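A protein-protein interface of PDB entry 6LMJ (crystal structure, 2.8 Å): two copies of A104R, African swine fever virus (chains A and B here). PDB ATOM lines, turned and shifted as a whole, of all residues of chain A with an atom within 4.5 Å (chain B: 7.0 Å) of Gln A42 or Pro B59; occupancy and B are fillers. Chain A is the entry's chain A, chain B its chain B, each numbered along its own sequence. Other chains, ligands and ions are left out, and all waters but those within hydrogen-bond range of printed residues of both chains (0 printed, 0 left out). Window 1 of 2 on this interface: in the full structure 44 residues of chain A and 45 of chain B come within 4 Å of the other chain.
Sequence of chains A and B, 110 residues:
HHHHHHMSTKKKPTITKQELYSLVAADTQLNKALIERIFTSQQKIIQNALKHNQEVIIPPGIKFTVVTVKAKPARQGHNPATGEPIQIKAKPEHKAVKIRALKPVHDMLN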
ATOM      1  N   LYS A  17     -14.465  17.256 -20.942  1.00  0.00           N
ATOM      2  CA  LYS A  17     -15.403  17.267 -22.066  1.00  0.00           C
ATOM      3  C   LYS A  17     -15.606  18.670 -22.625  1.00  0.00           C
ATOM      4  O   LYS A  17     -15.908  18.823 -23.813  1.00  0.00           O
ATOM      5  CB  LYS A  17     -16.748  16.647 -21.671  1.00  0.00           C
ATOM      6  CG  LYS A  17     -17.228  16.965 -20.273  1.00  0.00           C
ATOM      7  CD  LYS A  17     -18.510  16.199 -19.994  1.00  0.00           C
ATOM      8  CE  LYS A  17     -19.156  16.633 -18.692  1.00  0.00           C
ATOM      9  NZ  LYS A  17     -18.736  15.784 -17.547  1.00  0.00           N
ATOM     10  N   LEU A  20     -12.721  19.150 -24.702  1.00  0.00           N
ATOM     11  CA  LEU A  20     -12.914  18.203 -25.794  1.00  0.00           C
ATOM     12  C   LEU A  20     -13.831  18.784 -26.856  1.00  0.00           C
ATOM     13  O   LEU A  20     -13.581  18.607 -28.051  1.00  0.00           O
ATOM     14  CB  LEU A  20     -13.474  16.889 -25.259  1.00  0.00           C
ATOM     15  CG  LEU A  20     -14.058  15.922 -26.288  1.00  0.00           C
ATOM     16  CD1 LEU A  20     -12.950  15.191 -27.030  1.00  0.00           C
ATOM     17  CD2 LEU A  20     -14.984  14.942 -25.597  1.00  0.00           C
ATOM     18  N   TYR A  21     -14.897  19.477 -26.438  1.00  0.00           N
ATOM     19  CA  TYR A  21     -15.765  20.160 -27.395  1.00  0.00           C
ATOM     20  C   TYR A  21     -14.967  21.112 -28.276  1.00  0.00           C
ATOM     21  O   TYR A  21     -15.181  21.173 -29.492  1.00  0.00           O
ATOM     22  CB  TYR A  21     -16.870  20.926 -26.665  1.00  0.00           C
ATOM     23  CG  TYR A  21     -17.721  20.098 -25.728  1.00  0.00           C
ATOM     24  CD1 TYR A  21     -18.057  18.787 -26.034  1.00  0.00           C
ATOM     25  CD2 TYR A  21     -18.194  20.634 -24.534  1.00  0.00           C
ATOM     26  CE1 TYR A  21     -18.835  18.032 -25.176  1.00  0.00           C
ATOM     27  CE2 TYR A  21     -18.972  19.885 -23.672  1.00  0.00           C
ATOM     28  CZ  TYR A  21     -19.291  18.585 -23.998  1.00  0.00           C
ATOM     29  OH  TYR A  21     -20.066  17.836 -23.143  1.00  0.00           O
ATOM     30  N   ILE A  38     -25.131  18.523 -30.274  1.00  0.00           N
ATOM     31  CA  ILE A  38     -25.220  17.135 -30.713  1.00  0.00           C
ATOM     32  C   ILE A  38     -24.856  16.169 -29.590  1.00  0.00           C
ATOM     33  O   ILE A  38     -25.508  15.136 -29.421  1.00  0.00           O
ATOM     34  CB  ILE A  38     -24.330  16.934 -31.953  1.00  0.00           C
ATOM     35  CG1 ILE A  38     -24.748  17.918 -33.049  1.00  0.00           C
ATOM     36  CG2 ILE A  38     -24.403  15.495 -32.437  1.00  0.00           C
ATOM     37  CD1 ILE A  38     -24.332  17.518 -34.440  1.00  0.00           C
ATOM     38  N   PHE A  39     -23.820  16.484 -28.809  1.00  0.00           N
ATOM     39  CA  PHE A  39     -23.491  15.645 -27.660  1.00  0.00           C
ATOM     40  C   PHE A  39     -24.583  15.715 -26.599  1.00  0.00           C
ATOM     41  O   PHE A  39     -24.878  14.713 -25.938  1.00  0.00           O
ATOM     42  CB  PHE A  39     -22.142  16.059 -27.073  1.00  0.00           C
ATOM     43  CG  PHE A  39     -20.964  15.633 -27.903  1.00  0.00           C
ATOM     44  CD1 PHE A  39     -21.010  14.470 -28.652  1.00  0.00           C
ATOM     45  CD2 PHE A  39     -19.809  16.396 -27.932  1.00  0.00           C
ATOM     46  CE1 PHE A  39     -19.927  14.078 -29.415  1.00  0.00           C
ATOM     47  CE2 PHE A  39     -18.723  16.008 -28.692  1.00  0.00           C
ATOM     48  CZ  PHE A  39     -18.782  14.848 -29.434  1.00  0.00           C
ATOM     49  N   THR A  40     -25.188  16.893 -26.420  1.00  0.00           N
ATOM     50  CA  THR A  40     -26.353  17.001 -25.548  1.00  0.00           C
ATOM     51  C   THR A  40     -27.494  16.131 -26.059  1.00  0.00           C
ATOM     52  O   THR A  40     -28.162  15.444 -25.277  1.00  0.00           O
ATOM     53  CB  THR A  40     -26.797  18.460 -25.441  1.00  0.00           C
ATOM     54  OG1 THR A  40     -25.814  19.210 -24.717  1.00  0.00           O
ATOM     55  CG2 THR A  40     -28.138  18.568 -24.728  1.00  0.00           C
ATOM     56  N   SER A  41     -27.726  16.145 -27.373  1.00  0.00           N
ATOM     57  CA  SER A  41     -28.743  15.274 -27.955  1.00  0.00           C
ATOM     58  C   SER A  41     -28.388  13.808 -27.751  1.00  0.00           C
ATOM     59  O   SER A  41     -29.262  12.988 -27.450  1.00  0.00           O
ATOM     60  CB  SER A  41     -28.909  15.585 -29.440  1.00  0.00           C
ATOM     61  OG  SER A  41     -29.929  14.789 -30.017  1.00  0.00           O
ATOM     62  N   GLN A  42     -27.108  13.459 -27.911  1.00  0.00           N
ATOM     63  CA  GLN A  42     -26.677  12.092 -27.640  1.00  0.00           C
ATOM     64  C   GLN A  42     -26.938  11.706 -26.191  1.00  0.00           C
ATOM     65  O   GLN A  42     -27.273  10.551 -25.907  1.00  0.00           O
ATOM     66  CB  GLN A  42     -25.193  11.932 -27.976  1.00  0.00           C
ATOM     67  CG  GLN A  42     -24.663  10.517 -27.802  1.00  0.00           C
ATOM     68  CD  GLN A  42     -23.182  10.482 -27.477  1.00  0.00           C
ATOM     69  OE1 GLN A  42     -22.704  11.228 -26.623  1.00  0.00           O
ATOM     70  NE2 GLN A  42     -22.448   9.609 -28.157  1.00  0.00           N
ATOM     71  N   GLN A  43     -26.803  12.658 -25.265  1.00  0.00           N
ATOM     72  CA  GLN A  43     -27.099  12.375 -23.864  1.00  0.00           C
ATOM     73  C   GLN A  43     -28.587  12.122 -23.655  1.00  0.00           C
ATOM     74  O   GLN A  43     -28.970  11.286 -22.829  1.00  0.00           O
ATOM     75  CB  GLN A  43     -26.619  13.529 -22.986  1.00  0.00           C
ATOM     76  CG  GLN A  43     -26.811  13.302 -21.497  1.00  0.00           C
ATOM     77  CD  GLN A  43     -25.602  13.722 -20.685  1.00  0.00           C
ATOM     78  OE1 GLN A  43     -24.550  14.044 -21.237  1.00  0.00           O
ATOM     79  NE2 GLN A  43     -25.746  13.719 -19.364  1.00  0.00           N
ATOM     80  N   LYS A  44     -29.439  12.838 -24.391  1.00  0.00           N
ATOM     81  CA  LYS A  44     -30.878  12.615 -24.292  1.00  0.00           C
ATOM     82  C   LYS A  44     -31.250  11.217 -24.768  1.00  0.00           C
ATOM     83  O   LYS A  44     -31.987  10.491 -24.089  1.00  0.00           O
ATOM     84  CB  LYS A  44     -31.629  13.676 -25.098  1.00  0.00           C
ATOM     85  CG  LYS A  44     -33.144  13.573 -25.005  1.00  0.00           C
ATOM     86  CD  LYS A  44     -33.802  13.872 -26.344  1.00  0.00           C
ATOM     87  CE  LYS A  44     -33.579  15.316 -26.767  1.00  0.00           C
ATOM     88  NZ  LYS A  44     -34.456  16.258 -26.017  1.00  0.00           N
ATOM     89  N   ILE A  45     -30.747  10.822 -25.941  1.00  0.00           N
ATOM     90  CA  ILE A  45     -31.099   9.523 -26.513  1.00  0.00           C
ATOM     91  C   ILE A  45     -30.630   8.392 -25.605  1.00  0.00           C
ATOM     92  O   ILE A  45     -31.373   7.440 -25.338  1.00  0.00           O
ATOM     93  CB  ILE A  45     -30.514   9.383 -27.930  1.00  0.00           C
ATOM     94  CG1 ILE A  45     -30.829  10.620 -28.772  1.00  0.00           C
ATOM     95  CG2 ILE A  45     -31.047   8.128 -28.603  1.00  0.00           C
ATOM     96  CD1 ILE A  45     -32.307  10.913 -28.911  1.00  0.00           C
ATOM     97  N   ILE A  46     -29.385   8.475 -25.128  1.00  0.00           N
ATOM     98  CA  ILE A  46     -28.827   7.417 -24.286  1.00  0.00           C
ATOM     99  C   ILE A  46     -29.682   7.217 -23.041  1.00  0.00           C
ATOM    100  O   ILE A  46     -30.017   6.086 -22.668  1.00  0.00           O
ATOM    101  CB  ILE A  46     -27.368   7.739 -23.916  1.00  0.00           C
ATOM    102  CG1 ILE A  46     -26.456   7.615 -25.136  1.00  0.00           C
ATOM    103  CG2 ILE A  46     -26.884   6.821 -22.804  1.00  0.00           C
ATOM    104  CD1 ILE A  46     -25.068   8.169 -24.904  1.00  0.00           C
ATOM    105  N   ILE A  58     -22.444   3.487 -28.371  1.00  0.00           N
ATOM    106  CA  ILE A  58     -22.071   4.815 -28.847  1.00  0.00           C
ATOM    107  C   ILE A  58     -20.664   4.747 -29.424  1.00  0.00           C
ATOM    108  O   ILE A  58     -19.886   3.855 -29.053  1.00  0.00           O
ATOM    109  CB  ILE A  58     -22.154   5.858 -27.720  1.00  0.00           C
ATOM    110  CG1 ILE A  58     -20.949   5.730 -26.784  1.00  0.00           C
ATOM    111  CG2 ILE A  58     -23.438   5.693 -26.931  1.00  0.00           C
ATOM    112  CD1 ILE A  58     -20.882   6.800 -25.719  1.00  0.00           C
ATOM    113  N   LEU B  20     -27.908   5.013 -33.711  1.00  0.00           N
ATOM    114  CA  LEU B  20     -27.724   6.170 -32.841  1.00  0.00           C
ATOM    115  C   LEU B  20     -27.441   7.429 -33.647  1.00  0.00           C
ATOM    116  O   LEU B  20     -27.967   8.503 -33.331  1.00  0.00           O
ATOM    117  CB  LEU B  20     -26.597   5.909 -31.844  1.00  0.00           C
ATOM    118  CG  LEU B  20     -26.345   7.051 -30.858  1.00  0.00           C
ATOM    119  CD1 LEU B  20     -27.623   7.404 -30.109  1.00  0.00           C
ATOM    120  CD2 LEU B  20     -25.234   6.691 -29.891  1.00  0.00           C
ATOM    121  N   VAL B  24     -29.848  10.522 -33.348  1.00  0.00           N
ATOM    122  CA  VAL B  24     -29.411  11.874 -33.019  1.00  0.00           C
ATOM    123  C   VAL B  24     -29.683  12.826 -34.176  1.00  0.00           C
ATOM    124  O   VAL B  24     -30.148  13.952 -33.968  1.00  0.00           O
ATOM    125  CB  VAL B  24     -27.924  11.866 -32.623  1.00  0.00           C
ATOM    126  CG1 VAL B  24     -27.419  13.287 -32.424  1.00  0.00           C
ATOM    127  CG2 VAL B  24     -27.713  11.042 -31.362  1.00  0.00           C
ATOM    128  N   ASP B  27     -33.310  13.989 -34.134  1.00  0.00           N
ATOM    129  CA  ASP B  27     -33.649  14.882 -33.029  1.00  0.00           C
ATOM    130  C   ASP B  27     -33.115  16.290 -33.271  1.00  0.00           C
ATOM    131  O   ASP B  27     -33.842  17.278 -33.114  1.00  0.00           O
ATOM    132  CB  ASP B  27     -33.107  14.316 -31.716  1.00  0.00           C
ATOM    133  CG  ASP B  27     -33.408  15.208 -30.528  1.00  0.00           C
ATOM    134  OD1 ASP B  27     -34.578  15.621 -30.373  1.00  0.00           O
ATOM    135  OD2 ASP B  27     -32.475  15.499 -29.750  1.00  0.00           O
ATOM    136  N   THR B  28     -31.842  16.400 -33.656  1.00  0.00           N
ATOM    137  CA  THR B  28     -31.235  17.703 -33.896  1.00  0.00           C
ATOM    138  C   THR B  28     -31.718  18.360 -35.182  1.00  0.00           C
ATOM    139  O   THR B  28     -31.397  19.531 -35.410  1.00  0.00           O
ATOM    140  CB  THR B  28     -29.712  17.578 -33.946  1.00  0.00           C
ATOM    141  OG1 THR B  28     -29.338  16.702 -35.018  1.00  0.00           O
ATOM    142  CG2 THR B  28     -29.181  17.023 -32.641  1.00  0.00           C
ATOM    143  N   PHE B  39     -18.655  12.930 -34.900  1.00  0.00           N
ATOM    144  CA  PHE B  39     -18.255  11.803 -34.065  1.00  0.00           C
ATOM    145  C   PHE B  39     -16.957  11.168 -34.551  1.00  0.00           C
ATOM    146  O   PHE B  39     -16.156  10.693 -33.738  1.00  0.00           O
ATOM    147  CB  PHE B  39     -19.375  10.765 -34.016  1.00  0.00           C
ATOM    148  CG  PHE B  39     -20.382  11.015 -32.933  1.00  0.00           C
ATOM    149  CD1 PHE B  39     -20.025  10.902 -31.601  1.00  0.00           C
ATOM    150  CD2 PHE B  39     -21.683  11.372 -33.246  1.00  0.00           C
ATOM    151  CE1 PHE B  39     -20.946  11.127 -30.600  1.00  0.00           C
ATOM    152  CE2 PHE B  39     -22.610  11.604 -32.248  1.00  0.00           C
ATOM    153  CZ  PHE B  39     -22.240  11.482 -30.923  1.00  0.00           C
ATOM    154  N   GLN B  42     -14.175  13.255 -33.056  1.00  0.00           N
ATOM    155  CA  GLN B  42     -14.078  12.939 -31.635  1.00  0.00           C
ATOM    156  C   GLN B  42     -13.285  11.659 -31.421  1.00  0.00           C
ATOM    157  O   GLN B  42     -12.392  11.606 -30.570  1.00  0.00           O
ATOM    158  CB  GLN B  42     -15.472  12.807 -31.014  1.00  0.00           C
ATOM    159  CG  GLN B  42     -15.470  12.692 -29.494  1.00  0.00           C
ATOM    160  CD  GLN B  42     -16.483  11.683 -28.962  1.00  0.00           C
ATOM    161  OE1 GLN B  42     -16.490  10.519 -29.361  1.00  0.00           O
ATOM    162  NE2 GLN B  42     -17.331  12.129 -28.039  1.00  0.00           N
ATOM    163  N   ILE B  57     -11.988  12.753 -20.942  1.00  0.00           N
ATOM    164  CA  ILE B  57     -13.350  12.583 -20.452  1.00  0.00           C
ATOM    165  C   ILE B  57     -14.296  13.047 -21.549  1.00  0.00           C
ATOM    166  O   ILE B  57     -14.169  14.171 -22.048  1.00  0.00           O
ATOM    167  CB  ILE B  57     -13.594  13.364 -19.149  1.00  0.00           C
ATOM    168  CG1 ILE B  57     -12.553  12.980 -18.096  1.00  0.00           C
ATOM    169  CG2 ILE B  57     -15.001  13.111 -18.631  1.00  0.00           C
ATOM    170  CD1 ILE B  57     -12.538  13.894 -16.891  1.00  0.00           C
ATOM    171  N   ILE B  58     -15.230  12.184 -21.931  1.00  0.00           N
ATOM    172  CA  ILE B  58     -16.123  12.473 -23.052  1.00  0.00           C
ATOM    173  C   ILE B  58     -17.573  12.375 -22.592  1.00  0.00           C
ATOM    174  O   ILE B  58     -17.860  11.692 -21.598  1.00  0.00           O
ATOM    175  CB  ILE B  58     -15.862  11.524 -24.233  1.00  0.00           C
ATOM    176  CG1 ILE B  58     -16.312  10.106 -23.893  1.00  0.00           C
ATOM    177  CG2 ILE B  58     -14.392  11.527 -24.607  1.00  0.00           C
ATOM    178  CD1 ILE B  58     -16.363   9.194 -25.097  1.00  0.00           C
ATOM    179  N   PRO B  59     -18.510  13.041 -23.262  1.00  0.00           N
ATOM    180  CA  PRO B  59     -19.929  12.874 -22.924  1.00  0.00           C
ATOM    181  C   PRO B  59     -20.362  11.434 -23.121  1.00  0.00           C
ATOM    182  O   PRO B  59     -19.909  10.765 -24.063  1.00  0.00           O
ATOM    183  CB  PRO B  59     -20.645  13.812 -23.910  1.00  0.00           C
ATOM    184  CG  PRO B  59     -19.606  14.782 -24.342  1.00  0.00           C
ATOM    185  CD  PRO B  59     -18.313  14.032 -24.334  1.00  0.00           C
ATOM    186  N   PRO B  60     -21.254  10.915 -22.262  1.00  0.00           N
ATOM    187  CA  PRO B  60     -21.902  11.645 -21.170  1.00  0.00           C
ATOM    188  C   PRO B  60     -21.167  11.554 -19.834  1.00  0.00           C
ATOM    189  O   PRO B  60     -21.816  11.487 -18.790  1.00  0.00           O
ATOM    190  CB  PRO B  60     -23.258  10.955 -21.076  1.00  0.00           C
ATOM    191  CG  PRO B  60     -22.936   9.525 -21.390  1.00  0.00           C
ATOM    192  CD  PRO B  60     -21.788   9.548 -22.385  1.00  0.00           C
ATOM    193  N   GLY B  61     -19.838  11.566 -19.861  1.00  0.00           N
ATOM    194  CA  GLY B  61     -19.078  11.471 -18.630  1.00  0.00           C
ATOM    195  C   GLY B  61     -18.283  10.188 -18.497  1.00  0.00           C
ATOM    196  O   GLY B  61     -18.190   9.619 -17.406  1.00  0.00           O
ATOM    197  N   ILE B  62     -17.723   9.713 -19.607  1.00  0.00           N
ATOM    198  CA  ILE B  62     -16.867   8.533 -19.618  1.00  0.00           C
ATOM    199  C   ILE B  62     -15.419   8.988 -19.703  1.00  0.00           C
ATOM    200  O   ILE B  62     -15.068   9.808 -20.561  1.00  0.00           O
ATOM    201  CB  ILE B  62     -17.214   7.599 -20.789  1.00  0.00           C
ATOM    202  CG1 ILE B  62     -18.694   7.227 -20.763  1.00  0.00           C
ATOM    203  CG2 ILE B  62     -16.352   6.349 -20.741  1.00  0.00           C
ATOM    204  CD1 ILE B  62     -19.097   6.324 -21.900  1.00  0.00           C
ATOM    205  N   VAL B 105     -23.344   9.657 -15.604  1.00  0.00           N
ATOM    206  CA  VAL B 105     -23.712   8.355 -16.152  1.00  0.00           C
ATOM    207  C   VAL B 105     -24.629   7.608 -15.189  1.00  0.00           C
ATOM    208  O   VAL B 105     -25.685   7.104 -15.583  1.00  0.00           O
ATOM    209  CB  VAL B 105     -22.453   7.536 -16.492  1.00  0.00           C
ATOM    210  CG1 VAL B 105     -22.830   6.238 -17.188  1.00  0.00           C
ATOM    211  CG2 VAL B 105     -21.514   8.352 -17.363  1.00  0.00           C
ATOM    212  N   MET B 108     -28.111   9.072 -14.714  1.00  0.00           N
ATOM    213  CA  MET B 108     -29.023   8.933 -15.845  1.00  0.00           C
ATOM    214  C   MET B 108     -30.293   8.176 -15.485  1.00  0.00           C
ATOM    215  O   MET B 108     -31.309   8.339 -16.170  1.00  0.00           O
ATOM    216  CB  MET B 108     -28.319   8.228 -17.006  1.00  0.00           C
ATOM    217  CG  MET B 108     -27.465   9.141 -17.860  1.00  0.00           C
ATOM    218  SD  MET B 108     -26.764   8.271 -19.270  1.00  0.00           S
ATOM    219  CE  MET B 108     -26.529   9.630 -20.410  1.00  0.00           C
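The side-chain hydroxyl (OG1) of Thr B28 is in hydrogen-bond range of the backbone carbonyl oxygen (O) of Val B24.
Of the printed residues of chain B, Gln A42 touches Phe B39 (3.2 Å) and Pro B59 (3.8 Å). Pro B59 touches just these residues of chain A: Leu A20 (3.7 Å), Tyr A21 (3.3 Å), Phe A39 (3.9 Å) and Gln A42 (3.8 Å). Of the printed residues of chain B, Phe A39 touches Phe B39, Gln B42 and Pro B59. Of the printed residues of chain B, Ile A45 touches Leu B20. Of the printed residues of chain A, Asp B27 touches Ser A41 and Lys A44. Of the printed residues of chain B, Ile A46 touches Met B108 (3.7 Å). Printed residues of chain B within 4 Å of Ile A58: Leu B20 (3.6 Å). The nearest residue of chain A that does not touch Pro B59 is Lys A17 (4.05 Å). The nearest printed residue of chain A that does not touch Phe B39 is Ile A38 (4.3 Å).
The backbone NH (N) of Lys A17 lies within hydrogen-bond range of the backbone carbonyl oxygen (O) of Ile B57 (3.3 Å). The side-chain hydroxyl (OG) of Ser A41 is in hydrogen-bond range of the side-chain carboxylate (OD2) of Asp B27, 2.7 Å away.
Ile B57 touches Leu A20 (O to CD2, 3.7 Å). Leu A20 touches Ile B58. CD of Pro B59 touches CD2 of Leu A20, at 3.7 Å. OH of Tyr A21 touches CG of Pro B59, 3.3 Å away. CE1 of Phe A39 touches CE1 of Phe B39, at 3.3 Å. Gln B42 touches Phe A39 (NE2 to CZ, 3.4 Å). CB of Ser A41 touches CG2 of Thr B28, at 3.5 Å. Phe B39 touches Gln A42. Gln A42 touches Pro B59 (OE1 to O, 3.8 Å). CE of Met B108 touches O of Gln A43, at 3.8 Å.
Leu A20 touches Ile B58, and with the chains exchanged Ile A58 touches Leu B20. Phe B39 touches its own counterpart, Phe A39. Phe A39 touches Gln B42, and with the chains exchanged Gln A42 touches Phe B39.
Of the 14 printed residues of chain B, 11 touch a printed residue of chain A. Printed residues of chain B that touch a printed residue of chain A: Leu B20, Val B24, Asp B27, Thr B28, Phe B39, Gln B42, Ile B57, Ile B58, Pro B59, Pro B60 and Met B108. Hydrophobic or aromatic side chains of chain B within 4 Å of the printed part of chain A: Leu B20, Val B24, Phe B39, Ile B58, Pro B59, Pro B60 and Met B108. Among the printed residues, no Asp or Glu carboxylate lies within 4 Å of a Lys or Arg side-chain nitrogen of the other chain.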
